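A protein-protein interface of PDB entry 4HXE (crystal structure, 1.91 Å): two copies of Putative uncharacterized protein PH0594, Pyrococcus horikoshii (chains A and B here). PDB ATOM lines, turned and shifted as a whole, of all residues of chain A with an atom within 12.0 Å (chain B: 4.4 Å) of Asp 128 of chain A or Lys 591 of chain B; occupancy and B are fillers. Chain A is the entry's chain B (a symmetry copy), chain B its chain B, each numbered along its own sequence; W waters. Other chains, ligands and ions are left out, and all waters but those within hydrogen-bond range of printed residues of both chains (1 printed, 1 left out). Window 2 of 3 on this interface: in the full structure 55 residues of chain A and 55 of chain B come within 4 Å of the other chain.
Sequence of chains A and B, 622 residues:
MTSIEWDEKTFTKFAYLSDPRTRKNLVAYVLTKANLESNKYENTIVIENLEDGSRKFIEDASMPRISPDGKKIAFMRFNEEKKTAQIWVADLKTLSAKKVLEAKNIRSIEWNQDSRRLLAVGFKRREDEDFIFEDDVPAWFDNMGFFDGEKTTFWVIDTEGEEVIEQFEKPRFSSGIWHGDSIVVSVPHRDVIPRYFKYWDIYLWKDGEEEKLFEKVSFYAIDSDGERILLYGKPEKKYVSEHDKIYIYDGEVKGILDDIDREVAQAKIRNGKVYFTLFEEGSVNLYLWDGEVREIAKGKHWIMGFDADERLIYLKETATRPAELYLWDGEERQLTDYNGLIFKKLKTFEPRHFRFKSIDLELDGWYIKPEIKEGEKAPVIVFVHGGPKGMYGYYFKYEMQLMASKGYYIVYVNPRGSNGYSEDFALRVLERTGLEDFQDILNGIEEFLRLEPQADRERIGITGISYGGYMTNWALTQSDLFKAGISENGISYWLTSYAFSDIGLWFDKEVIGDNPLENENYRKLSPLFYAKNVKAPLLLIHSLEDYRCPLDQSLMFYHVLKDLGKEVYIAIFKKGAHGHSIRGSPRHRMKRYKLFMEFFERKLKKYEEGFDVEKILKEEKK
The backbone carbonyl oxygen (O) of Asp 128 of chain A is in hydrogen-bond range of the side-chain amino group (NZ) of Lys 574 of chain B (3.2 Å). N of Lys 574 of chain B sits at hydrogen-bond distance from O of Asp 130 of chain A (2.9 Å). The guanidinium group (NH2) of Arg 587 of chain B is in salt-bridge range of the side-chain carboxylate (OE1) of Glu 129 of chain A (2.8 Å). OD2 of Asp 130 of chain A lies within salt-bridge range of NE of Arg 587 of chain B (2.8 Å). NZ of Lys 591 of chain B is in salt-bridge range of OD1 of Asp 128 of chain A, at 2.7 Å. The side-chain amino group (NZ) of Lys 591 of chain B lies within salt-bridge range of the side-chain carboxylate (OD2) of Asp 130 of chain A, 2.9 Å away.
The side-chain carboxylate of Asp 128 of chain A is in hydrogen-bond range of the backbone NH of Asp 130 of chain A, 2.7 Å away. OD2 of Asp 128 of chain A lies within hydrogen-bond range of N of Phe 131 of chain A, 3.1 Å away.
Glu 129 of chain A touches Lys 574 of chain B. Asp 130 of chain A touches His 588 of chain B (OD2 to N, 3.9 Å). Phe 131 of chain A touches Lys 591 of chain B. Phe 131 of chain A touches Leu 595 of chain B. Leu 617 of chain B touches Phe 131 of chain A (CD2 to CZ, 3.9 Å). CG of Lys 574 of chain B touches CD1 of Ile 132 of chain A, at 3.8 Å.
Asp 128 of chain A touches just these residues of chain B: Lys 574 (3.2 Å) and Lys 591 (2.7 Å). Of the printed residues of chain A, Leu 595 of chain B touches Phe 131 (3.9 Å). Of the printed residues of chain A, Arg 587 of chain B touches Glu 129 and Asp 130. Of the printed residues of chain A, Leu 617 of chain B touches Phe 131. Printed residues of chain B within 4 Å of Glu 129 of chain A: Lys 574 (3.7 Å) and Arg 587 (2.8 Å). Arg 125 of chain A touches none of the printed residues of chain B. The nearest printed residue of chain B that does not touch Asp 128 of chain A is Leu 617 of chain B (5.9 Å). The nearest printed residue of chain A that does not touch Lys 591 of chain B is Glu 129 of chain A (4.2 Å). The nearest printed residue of chain A that does not touch Lys 574 of chain B is Phe 131 of chain A (4.3 Å).
Of the 11 printed residues of chain B, 6 touch a printed residue of chain A. Hydrophobic or aromatic side chains of chain B that line the printed part of chain A: Leu 595 and Leu 617. Of the 18 printed residues of chain A, 5 touch a printed residue of chain B. Hydrophobic or aromatic side chains of chain A within 4 Å of the printed part of chain B: Phe 131 and Ile 132. Among the printed residues, 12 pairs touch across the chains.
No position is printed for both chains.
Water W1 lies within hydrogen-bond range of a ring nitrogen (ND1) of His 588 of chain B (2.7 Å), the backbone carbonyl oxygen (O) of Asp 130 of chain A (2.8 Å) and the backbone NH (N) of Lys 574 of chain B (3.4 Å).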
ATOM      1  N   ASN A 105      16.896 -37.112  -7.727  1.00  0.00           N
ATOM      2  CA  ASN A 105      17.746 -36.340  -6.816  1.00  0.00           C
ATOM      3  C   ASN A 105      18.020 -36.948  -5.474  1.00  0.00           C
ATOM      4  O   ASN A 105      18.098 -36.225  -4.473  1.00  0.00           O
ATOM      5  CB  ASN A 105      17.206 -34.908  -6.653  1.00  0.00           C
ATOM      6  CG  ASN A 105      16.968 -34.231  -7.997  1.00  0.00           C
ATOM      7  OD1 ASN A 105      17.715 -34.432  -8.969  1.00  0.00           O
ATOM      8  ND2 ASN A 105      15.933 -33.448  -8.059  1.00  0.00           N
ATOM      9  N   PHE A 123      17.981 -33.868  -2.532  1.00  0.00           N
ATOM     10  CA  PHE A 123      18.010 -32.431  -2.595  1.00  0.00           C
ATOM     11  C   PHE A 123      16.819 -31.988  -3.407  1.00  0.00           C
ATOM     12  O   PHE A 123      16.277 -32.778  -4.127  1.00  0.00           O
ATOM     13  CB  PHE A 123      19.349 -31.920  -3.206  1.00  0.00           C
ATOM     14  CG  PHE A 123      19.602 -32.357  -4.637  1.00  0.00           C
ATOM     15  CD1 PHE A 123      20.271 -33.559  -4.902  1.00  0.00           C
ATOM     16  CD2 PHE A 123      19.169 -31.590  -5.718  1.00  0.00           C
ATOM     17  CE1 PHE A 123      20.548 -33.965  -6.219  1.00  0.00           C
ATOM     18  CE2 PHE A 123      19.445 -31.985  -7.047  1.00  0.00           C
ATOM     19  CZ  PHE A 123      20.130 -33.176  -7.293  1.00  0.00           C
ATOM     20  N   LYS A 124      16.422 -30.732  -3.250  1.00  0.00           N
ATOM     21  CA  LYS A 124      15.425 -30.097  -4.102  1.00  0.00           C
ATOM     22  C   LYS A 124      15.846 -28.671  -4.450  1.00  0.00           C
ATOM     23  O   LYS A 124      16.401 -27.968  -3.601  1.00  0.00           O
ATOM     24  CB  LYS A 124      14.015 -30.138  -3.458  1.00  0.00           C
ATOM     25  CG  LYS A 124      13.830 -29.381  -2.149  1.00  0.00           C
ATOM     26  CD  LYS A 124      12.397 -29.572  -1.610  1.00  0.00           C
ATOM     27  N   ARG A 125      15.529 -28.226  -5.673  1.00  0.00           N
ATOM     28  CA  ARG A 125      15.910 -26.878  -6.166  1.00  0.00           C
ATOM     29  C   ARG A 125      14.672 -26.147  -6.742  1.00  0.00           C
ATOM     30  O   ARG A 125      13.599 -26.755  -6.882  1.00  0.00           O
ATOM     31  CB  ARG A 125      16.966 -27.058  -7.258  1.00  0.00           C
ATOM     32  CG  ARG A 125      18.107 -27.979  -6.845  1.00  0.00           C
ATOM     33  CD  ARG A 125      19.186 -27.961  -7.944  1.00  0.00           C
ATOM     34  NE  ARG A 125      20.427 -28.557  -7.459  1.00  0.00           N
ATOM     35  CZ  ARG A 125      21.407 -29.061  -8.227  1.00  0.00           C
ATOM     36  NH1 ARG A 125      21.310 -29.021  -9.560  1.00  0.00           N
ATOM     37  NH2 ARG A 125      22.489 -29.630  -7.669  1.00  0.00           N
ATOM     38  N   ARG A 126      14.825 -24.892  -7.139  1.00  0.00           N
ATOM     39  CA  ARG A 126      13.678 -24.111  -7.677  1.00  0.00           C
ATOM     40  C   ARG A 126      13.202 -24.659  -9.033  1.00  0.00           C
ATOM     41  O   ARG A 126      12.029 -24.831  -9.227  1.00  0.00           O
ATOM     42  CB  ARG A 126      14.054 -22.646  -7.708  1.00  0.00           C
ATOM     43  CG  ARG A 126      14.103 -22.008  -6.307  1.00  0.00           C
ATOM     44  CD  ARG A 126      14.676 -20.579  -6.349  1.00  0.00           C
ATOM     45  NE  ARG A 126      14.580 -20.055  -4.979  1.00  0.00           N
ATOM     46  CZ  ARG A 126      15.618 -19.658  -4.222  1.00  0.00           C
ATOM     47  NH1 ARG A 126      15.410 -19.252  -2.964  1.00  0.00           N
ATOM     48  NH2 ARG A 126      16.869 -19.657  -4.702  1.00  0.00           N
ATOM     49  N   GLU A 127      14.109 -24.942  -9.961  1.00  0.00           N
ATOM     50  CA  GLU A 127      13.792 -25.660 -11.210  1.00  0.00           C
ATOM     51  C   GLU A 127      12.962 -24.912 -12.252  1.00  0.00           C
ATOM     52  O   GLU A 127      12.327 -25.526 -13.128  1.00  0.00           O
ATOM     53  CB  GLU A 127      13.213 -27.066 -10.928  1.00  0.00           C
ATOM     54  CG  GLU A 127      14.261 -28.017 -10.355  1.00  0.00           C
ATOM     55  CD  GLU A 127      13.742 -29.433 -10.213  1.00  0.00           C
ATOM     56  OE1 GLU A 127      12.517 -29.643 -10.324  1.00  0.00           O
ATOM     57  OE2 GLU A 127      14.561 -30.335 -10.013  1.00  0.00           O
ATOM     58  N   ASP A 128      12.987 -23.583 -12.202  1.00  0.00           N
ATOM     59  CA  ASP A 128      12.396 -22.850 -13.300  1.00  0.00           C
ATOM     60  C   ASP A 128      13.168 -23.198 -14.597  1.00  0.00           C
ATOM     61  O   ASP A 128      14.435 -23.308 -14.584  1.00  0.00           O
ATOM     62  CB  ASP A 128      12.418 -21.390 -13.056  1.00  0.00           C
ATOM     63  CG  ASP A 128      11.810 -20.641 -14.207  1.00  0.00           C
ATOM     64  OD1 ASP A 128      10.597 -20.450 -14.199  1.00  0.00           O
ATOM     65  OD2 ASP A 128      12.513 -20.366 -15.183  1.00  0.00           O
ATOM     66  N   GLU A 129      12.424 -23.390 -15.704  1.00  0.00           N
ATOM     67  CA  GLU A 129      13.081 -23.919 -16.890  1.00  0.00           C
ATOM     68  C   GLU A 129      13.883 -22.849 -17.596  1.00  0.00           C
ATOM     69  O   GLU A 129      14.716 -23.174 -18.383  1.00  0.00           O
ATOM     70  CB  GLU A 129      12.113 -24.620 -17.865  1.00  0.00           C
ATOM     71  CG  GLU A 129      11.017 -23.718 -18.421  1.00  0.00           C
ATOM     72  CD  GLU A 129      10.125 -24.473 -19.395  1.00  0.00           C
ATOM     73  OE1 GLU A 129      10.641 -25.038 -20.381  1.00  0.00           O
ATOM     74  OE2 GLU A 129       8.909 -24.512 -19.151  1.00  0.00           O
ATOM     75  N   ASP A 130      13.681 -21.580 -17.262  1.00  0.00           N
ATOM     76  CA  ASP A 130      14.414 -20.504 -17.932  1.00  0.00           C
ATOM     77  C   ASP A 130      15.567 -19.870 -17.180  1.00  0.00           C
ATOM     78  O   ASP A 130      16.498 -19.370 -17.808  1.00  0.00           O
ATOM     79  CB  ASP A 130      13.458 -19.420 -18.369  1.00  0.00           C
ATOM     80  CG  ASP A 130      12.459 -19.942 -19.339  1.00  0.00           C
ATOM     81  OD1 ASP A 130      12.866 -20.583 -20.321  1.00  0.00           O
ATOM     82  OD2 ASP A 130      11.275 -19.777 -19.099  1.00  0.00           O
ATOM     83  N   PHE A 131      15.522 -19.868 -15.853  1.00  0.00           N
ATOM     84  CA  PHE A 131      16.575 -19.184 -15.068  1.00  0.00           C
ATOM     85  C   PHE A 131      16.747 -19.901 -13.714  1.00  0.00           C
ATOM     86  O   PHE A 131      15.794 -20.499 -13.172  1.00  0.00           O
ATOM     87  CB  PHE A 131      16.354 -17.657 -14.922  1.00  0.00           C
ATOM     88  CG  PHE A 131      15.184 -17.272 -13.985  1.00  0.00           C
ATOM     89  CD1 PHE A 131      13.858 -17.237 -14.463  1.00  0.00           C
ATOM     90  CD2 PHE A 131      15.419 -16.992 -12.636  1.00  0.00           C
ATOM     91  CE1 PHE A 131      12.800 -16.945 -13.604  1.00  0.00           C
ATOM     92  CE2 PHE A 131      14.371 -16.691 -11.763  1.00  0.00           C
ATOM     93  CZ  PHE A 131      13.036 -16.695 -12.253  1.00  0.00           C
ATOM     94  N   ILE A 132      17.993 -19.881 -13.259  1.00  0.00           N
ATOM     95  CA  ILE A 132      18.430 -20.285 -11.949  1.00  0.00           C
ATOM     96  C   ILE A 132      18.272 -19.020 -11.125  1.00  0.00           C
ATOM     97  O   ILE A 132      18.486 -17.907 -11.643  1.00  0.00           O
ATOM     98  CB  ILE A 132      19.937 -20.676 -12.012  1.00  0.00           C
ATOM     99  CG1 ILE A 132      20.058 -21.957 -12.885  1.00  0.00           C
ATOM    100  CG2 ILE A 132      20.541 -20.904 -10.615  1.00  0.00           C
ATOM    101  CD1 ILE A 132      21.074 -21.715 -14.012  1.00  0.00           C
ATOM    102  N   PHE A 133      17.827 -19.185  -9.882  1.00  0.00           N
ATOM    103  CA  PHE A 133      17.747 -18.036  -8.982  1.00  0.00           C
ATOM    104  C   PHE A 133      18.459 -18.346  -7.659  1.00  0.00           C
ATOM    105  O   PHE A 133      18.189 -19.376  -7.041  1.00  0.00           O
ATOM    106  CB  PHE A 133      16.300 -17.610  -8.738  1.00  0.00           C
ATOM    107  CG  PHE A 133      16.206 -16.318  -7.977  1.00  0.00           C
ATOM    108  CD1 PHE A 133      16.377 -15.098  -8.621  1.00  0.00           C
ATOM    109  CD2 PHE A 133      16.070 -16.327  -6.569  1.00  0.00           C
ATOM    110  CE1 PHE A 133      16.342 -13.919  -7.904  1.00  0.00           C
ATOM    111  CE2 PHE A 133      16.040 -15.131  -5.849  1.00  0.00           C
ATOM    112  CZ  PHE A 133      16.161 -13.932  -6.529  1.00  0.00           C
ATOM    113  N   GLU A 134      19.397 -17.492  -7.263  1.00  0.00           N
ATOM    114  CA  GLU A 134      20.235 -17.776  -6.094  1.00  0.00           C
ATOM    115  C   GLU A 134      20.215 -16.649  -5.045  1.00  0.00           C
ATOM    116  O   GLU A 134      20.352 -15.478  -5.378  1.00  0.00           O
ATOM    117  CB  GLU A 134      21.693 -18.017  -6.518  1.00  0.00           C
ATOM    118  CG  GLU A 134      22.530 -18.655  -5.377  1.00  0.00           C
ATOM    119  CD  GLU A 134      21.883 -19.880  -4.730  1.00  0.00           C
ATOM    120  OE1 GLU A 134      21.593 -19.772  -3.527  1.00  0.00           O
ATOM    121  OE2 GLU A 134      21.646 -20.963  -5.388  1.00  0.00           O
ATOM    122  N   PHE A 146      24.306 -25.884 -10.919  1.00  0.00           N
ATOM    123  CA  PHE A 146      23.906 -24.703 -10.170  1.00  0.00           C
ATOM    124  C   PHE A 146      22.997 -25.104  -9.032  1.00  0.00           C
ATOM    125  O   PHE A 146      22.078 -25.921  -9.239  1.00  0.00           O
ATOM    126  CB  PHE A 146      23.111 -23.769 -11.086  1.00  0.00           C
ATOM    127  CG  PHE A 146      23.973 -23.082 -12.091  1.00  0.00           C
ATOM    128  CD1 PHE A 146      24.281 -23.696 -13.310  1.00  0.00           C
ATOM    129  CD2 PHE A 146      24.526 -21.836 -11.802  1.00  0.00           C
ATOM    130  CE1 PHE A 146      25.091 -23.042 -14.238  1.00  0.00           C
ATOM    131  CE2 PHE A 146      25.332 -21.210 -12.721  1.00  0.00           C
ATOM    132  CZ  PHE A 146      25.602 -21.803 -13.957  1.00  0.00           C
ATOM    133  N   PHE A 147      23.145 -24.448  -7.875  1.00  0.00           N
ATOM    134  CA  PHE A 147      22.372 -24.881  -6.747  1.00  0.00           C
ATOM    135  C   PHE A 147      20.916 -24.528  -6.913  1.00  0.00           C
ATOM    136  O   PHE A 147      20.050 -25.255  -6.446  1.00  0.00           O
ATOM    137  CB  PHE A 147      22.913 -24.377  -5.406  1.00  0.00           C
ATOM    138  CG  PHE A 147      24.014 -25.265  -4.818  1.00  0.00           C
ATOM    139  CD1 PHE A 147      25.257 -24.725  -4.459  1.00  0.00           C
ATOM    140  CD2 PHE A 147      23.793 -26.612  -4.630  1.00  0.00           C
ATOM    141  CE1 PHE A 147      26.253 -25.505  -3.868  1.00  0.00           C
ATOM    142  CE2 PHE A 147      24.770 -27.431  -4.041  1.00  0.00           C
ATOM    143  CZ  PHE A 147      26.002 -26.861  -3.643  1.00  0.00           C
ATOM    144  N   ASP A 148      20.653 -23.377  -7.495  1.00  0.00           N
ATOM    145  CA  ASP A 148      19.291 -22.960  -7.730  1.00  0.00           C
ATOM    146  C   ASP A 148      18.431 -23.056  -6.459  1.00  0.00           C
ATOM    147  O   ASP A 148      17.297 -23.619  -6.467  1.00  0.00           O
ATOM    148  CB  ASP A 148      18.717 -23.770  -8.912  1.00  0.00           C
ATOM    149  CG  ASP A 148      17.447 -23.150  -9.495  1.00  0.00           C
ATOM    150  OD1 ASP A 148      17.124 -21.934  -9.296  1.00  0.00           O
ATOM    151  OD2 ASP A 148      16.724 -23.961 -10.076  1.00  0.00           O
ATOM    152  N   GLY A 149      18.982 -22.521  -5.363  1.00  0.00           N
ATOM    153  CA  GLY A 149      18.236 -22.470  -4.086  1.00  0.00           C
ATOM    154  C   GLY A 149      18.189 -23.819  -3.383  1.00  0.00           C
ATOM    155  O   GLY A 149      17.408 -23.978  -2.443  1.00  0.00           O
ATOM    156  N   GLU A 150      19.039 -24.783  -3.808  1.00  0.00           N
ATOM    157  CA  GLU A 150      19.023 -26.157  -3.261  1.00  0.00           C
ATOM    158  C   GLU A 150      18.870 -26.297  -1.720  1.00  0.00           C
ATOM    159  O   GLU A 150      19.637 -25.699  -0.920  1.00  0.00           O
ATOM    160  CB  GLU A 150      20.278 -26.897  -3.702  1.00  0.00           C
ATOM    161  CG  GLU A 150      20.320 -28.346  -3.180  1.00  0.00           C
ATOM    162  CD  GLU A 150      21.467 -29.181  -3.757  1.00  0.00           C
ATOM    163  OE1 GLU A 150      21.705 -29.164  -4.993  1.00  0.00           O
ATOM    164  OE2 GLU A 150      22.144 -29.873  -2.938  1.00  0.00           O
ATOM    165  N   LYS B 574      19.341 -19.455 -18.376  1.00  0.00           N
ATOM    166  CA  LYS B 574      20.097 -20.640 -18.773  1.00  0.00           C
ATOM    167  C   LYS B 574      20.411 -20.540 -20.228  1.00  0.00           C
ATOM    168  O   LYS B 574      21.350 -21.138 -20.649  1.00  0.00           O
ATOM    169  CB  LYS B 574      19.308 -21.918 -18.538  1.00  0.00           C
ATOM    170  CG  LYS B 574      18.949 -22.164 -17.091  1.00  0.00           C
ATOM    171  CD  LYS B 574      18.120 -23.440 -17.032  1.00  0.00           C
ATOM    172  CE  LYS B 574      17.761 -23.716 -15.596  1.00  0.00           C
ATOM    173  NZ  LYS B 574      16.925 -24.960 -15.593  1.00  0.00           N
ATOM    174  N   ARG B 587       9.182 -16.559 -23.439  1.00  0.00           N
ATOM    175  CA  ARG B 587       8.926 -16.982 -22.044  1.00  0.00           C
ATOM    176  C   ARG B 587      10.059 -16.509 -21.153  1.00  0.00           C
ATOM    177  O   ARG B 587       9.819 -15.927 -20.124  1.00  0.00           O
ATOM    178  CB  ARG B 587       8.841 -18.520 -21.914  1.00  0.00           C
ATOM    179  CG  ARG B 587       7.999 -18.944 -20.696  1.00  0.00           C
ATOM    180  CD  ARG B 587       7.927 -20.479 -20.551  1.00  0.00           C
ATOM    181  NE  ARG B 587       9.314 -21.030 -20.619  1.00  0.00           N
ATOM    182  CZ  ARG B 587       9.678 -22.048 -21.410  1.00  0.00           C
ATOM    183  NH1 ARG B 587       8.773 -22.672 -22.167  1.00  0.00           N
ATOM    184  NH2 ARG B 587      10.921 -22.469 -21.452  1.00  0.00           N
ATOM    185  N   HIS B 588      11.304 -16.745 -21.575  1.00  0.00           N
ATOM    186  CA  HIS B 588      12.485 -16.174 -20.946  1.00  0.00           C
ATOM    187  C   HIS B 588      12.329 -14.663 -20.700  1.00  0.00           C
ATOM    188  O   HIS B 588      12.494 -14.183 -19.589  1.00  0.00           O
ATOM    189  CB  HIS B 588      13.685 -16.533 -21.845  1.00  0.00           C
ATOM    190  CG  HIS B 588      14.986 -15.805 -21.522  1.00  0.00           C
ATOM    191  ND1 HIS B 588      16.216 -16.416 -21.609  1.00  0.00           N
ATOM    192  CD2 HIS B 588      15.231 -14.458 -21.239  1.00  0.00           C
ATOM    193  CE1 HIS B 588      17.188 -15.518 -21.336  1.00  0.00           C
ATOM    194  NE2 HIS B 588      16.596 -14.311 -21.103  1.00  0.00           N
ATOM    195  N   ARG B 589      11.975 -13.901 -21.742  1.00  0.00           N
ATOM    196  CA  ARG B 589      11.840 -12.458 -21.606  1.00  0.00           C
ATOM    197  C   ARG B 589      10.715 -12.039 -20.698  1.00  0.00           C
ATOM    198  O   ARG B 589      10.886 -11.157 -19.900  1.00  0.00           O
ATOM    199  CB  ARG B 589      11.670 -11.818 -22.980  1.00  0.00           C
ATOM    200  CG  ARG B 589      12.944 -11.903 -23.836  1.00  0.00           C
ATOM    201  CD  ARG B 589      12.625 -11.288 -25.200  1.00  0.00           C
ATOM    202  NE  ARG B 589      12.289  -9.852 -25.067  1.00  0.00           N
ATOM    203  CZ  ARG B 589      11.675  -9.155 -26.025  1.00  0.00           C
ATOM    204  NH1 ARG B 589      11.295  -9.787 -27.125  1.00  0.00           N
ATOM    205  NH2 ARG B 589      11.387  -7.879 -25.867  1.00  0.00           N
ATOM    206  N   MET B 590       9.576 -12.669 -20.817  1.00  0.00           N
ATOM    207  CA  MET B 590       8.460 -12.422 -19.887  1.00  0.00           C
ATOM    208  C   MET B 590       8.923 -12.603 -18.428  1.00  0.00           C
ATOM    209  O   MET B 590       8.610 -11.797 -17.550  1.00  0.00           O
ATOM    210  CB  MET B 590       7.261 -13.323 -20.236  1.00  0.00           C
ATOM    211  CG  MET B 590       6.026 -13.120 -19.349  1.00  0.00           C
ATOM    212  SD  MET B 590       6.153 -14.221 -17.909  1.00  0.00           S
ATOM    213  CE  MET B 590       5.929 -15.856 -18.623  1.00  0.00           C
ATOM    214  N   LYS B 591       9.694 -13.648 -18.161  1.00  0.00           N
ATOM    215  CA  LYS B 591      10.143 -13.902 -16.755  1.00  0.00           C
ATOM    216  C   LYS B 591      11.100 -12.839 -16.264  1.00  0.00           C
ATOM    217  O   LYS B 591      10.923 -12.321 -15.175  1.00  0.00           O
ATOM    218  CB  LYS B 591      10.743 -15.313 -16.565  1.00  0.00           C
ATOM    219  CG  LYS B 591       9.628 -16.391 -16.559  1.00  0.00           C
ATOM    220  CD  LYS B 591      10.213 -17.794 -16.604  1.00  0.00           C
ATOM    221  CE  LYS B 591       9.070 -18.819 -16.731  1.00  0.00           C
ATOM    222  NZ  LYS B 591       9.699 -20.141 -16.743  1.00  0.00           N
ATOM    223  N   ARG B 592      12.037 -12.422 -17.119  1.00  0.00           N
ATOM    224  CA  ARG B 592      12.907 -11.300 -16.787  1.00  0.00           C
ATOM    225  C   ARG B 592      12.099 -10.014 -16.517  1.00  0.00           C
ATOM    226  O   ARG B 592      12.383  -9.319 -15.521  1.00  0.00           O
ATOM    227  CB  ARG B 592      13.946 -11.043 -17.876  1.00  0.00           C
ATOM    228  CG  ARG B 592      14.764  -9.804 -17.560  1.00  0.00           C
ATOM    229  CD  ARG B 592      15.718  -9.443 -18.681  1.00  0.00           C
ATOM    230  NE  ARG B 592      16.185  -8.092 -18.433  1.00  0.00           N
ATOM    231  CZ  ARG B 592      15.483  -6.993 -18.768  1.00  0.00           C
ATOM    232  NH1 ARG B 592      15.960  -5.779 -18.548  1.00  0.00           N
ATOM    233  NH2 ARG B 592      14.339  -7.128 -19.414  1.00  0.00           N
ATOM    234  N   TYR B 593      11.123  -9.686 -17.372  1.00  0.00           N
ATOM    235  CA  TYR B 593      10.348  -8.465 -17.134  1.00  0.00           C
ATOM    236  C   TYR B 593       9.631  -8.509 -15.822  1.00  0.00           C
ATOM    237  O   TYR B 593       9.617  -7.519 -15.064  1.00  0.00           O
ATOM    238  CB  TYR B 593       9.365  -8.169 -18.262  1.00  0.00           C
ATOM    239  CG  TYR B 593      10.002  -7.761 -19.567  1.00  0.00           C
ATOM    240  CD1 TYR B 593       9.621  -8.413 -20.776  1.00  0.00           C
ATOM    241  CD2 TYR B 593      10.987  -6.755 -19.626  1.00  0.00           C
ATOM    242  CE1 TYR B 593      10.156  -8.044 -21.971  1.00  0.00           C
ATOM    243  CE2 TYR B 593      11.516  -6.356 -20.865  1.00  0.00           C
ATOM    244  CZ  TYR B 593      11.108  -7.032 -22.013  1.00  0.00           C
ATOM    245  OH  TYR B 593      11.624  -6.704 -23.242  1.00  0.00           O
ATOM    246  N   LYS B 594       9.034  -9.657 -15.539  1.00  0.00           N
ATOM    247  CA  LYS B 594       8.339  -9.877 -14.258  1.00  0.00           C
ATOM    248  C   LYS B 594       9.303  -9.697 -13.043  1.00  0.00           C
ATOM    249  O   LYS B 594       8.967  -8.976 -12.114  1.00  0.00           O
ATOM    250  CB  LYS B 594       7.713 -11.246 -14.203  1.00  0.00           C
ATOM    251  CG  LYS B 594       6.897 -11.546 -12.935  1.00  0.00           C
ATOM    252  CD  LYS B 594       5.958 -10.427 -12.485  1.00  0.00           C
ATOM    253  CE  LYS B 594       4.737 -10.937 -11.727  1.00  0.00           C
ATOM    254  NZ  LYS B 594       3.935  -9.719 -11.342  1.00  0.00           N
ATOM    255  N   LEU B 595      10.459 -10.343 -13.068  1.00  0.00           N
ATOM    256  CA  LEU B 595      11.464 -10.171 -12.006  1.00  0.00           C
ATOM    257  C   LEU B 595      11.845  -8.705 -11.827  1.00  0.00           C
ATOM    258  O   LEU B 595      12.011  -8.214 -10.728  1.00  0.00           O
ATOM    259  CB  LEU B 595      12.799 -10.837 -12.416  1.00  0.00           C
ATOM    260  CG  LEU B 595      12.832 -12.298 -12.066  1.00  0.00           C
ATOM    261  CD1 LEU B 595      13.877 -12.994 -12.924  1.00  0.00           C
ATOM    262  CD2 LEU B 595      13.199 -12.349 -10.578  1.00  0.00           C
ATOM    263  N   LEU B 617       6.750 -14.946  -8.744  1.00  0.00           N
ATOM    264  CA  LEU B 617       6.505 -15.196 -10.172  1.00  0.00           C
ATOM    265  C   LEU B 617       5.283 -16.078 -10.485  1.00  0.00           C
ATOM    266  O   LEU B 617       4.671 -15.907 -11.528  1.00  0.00           O
ATOM    267  CB  LEU B 617       7.795 -15.647 -10.910  1.00  0.00           C
ATOM    268  CG  LEU B 617       8.654 -14.462 -11.423  1.00  0.00           C
ATOM    269  CD1 LEU B 617       9.365 -13.632 -10.336  1.00  0.00           C
ATOM    270  CD2 LEU B 617       9.631 -14.890 -12.517  1.00  0.00           C
HETATM  271  O   HOH W   1      16.731 -18.759 -20.482  1.00  0.00           O
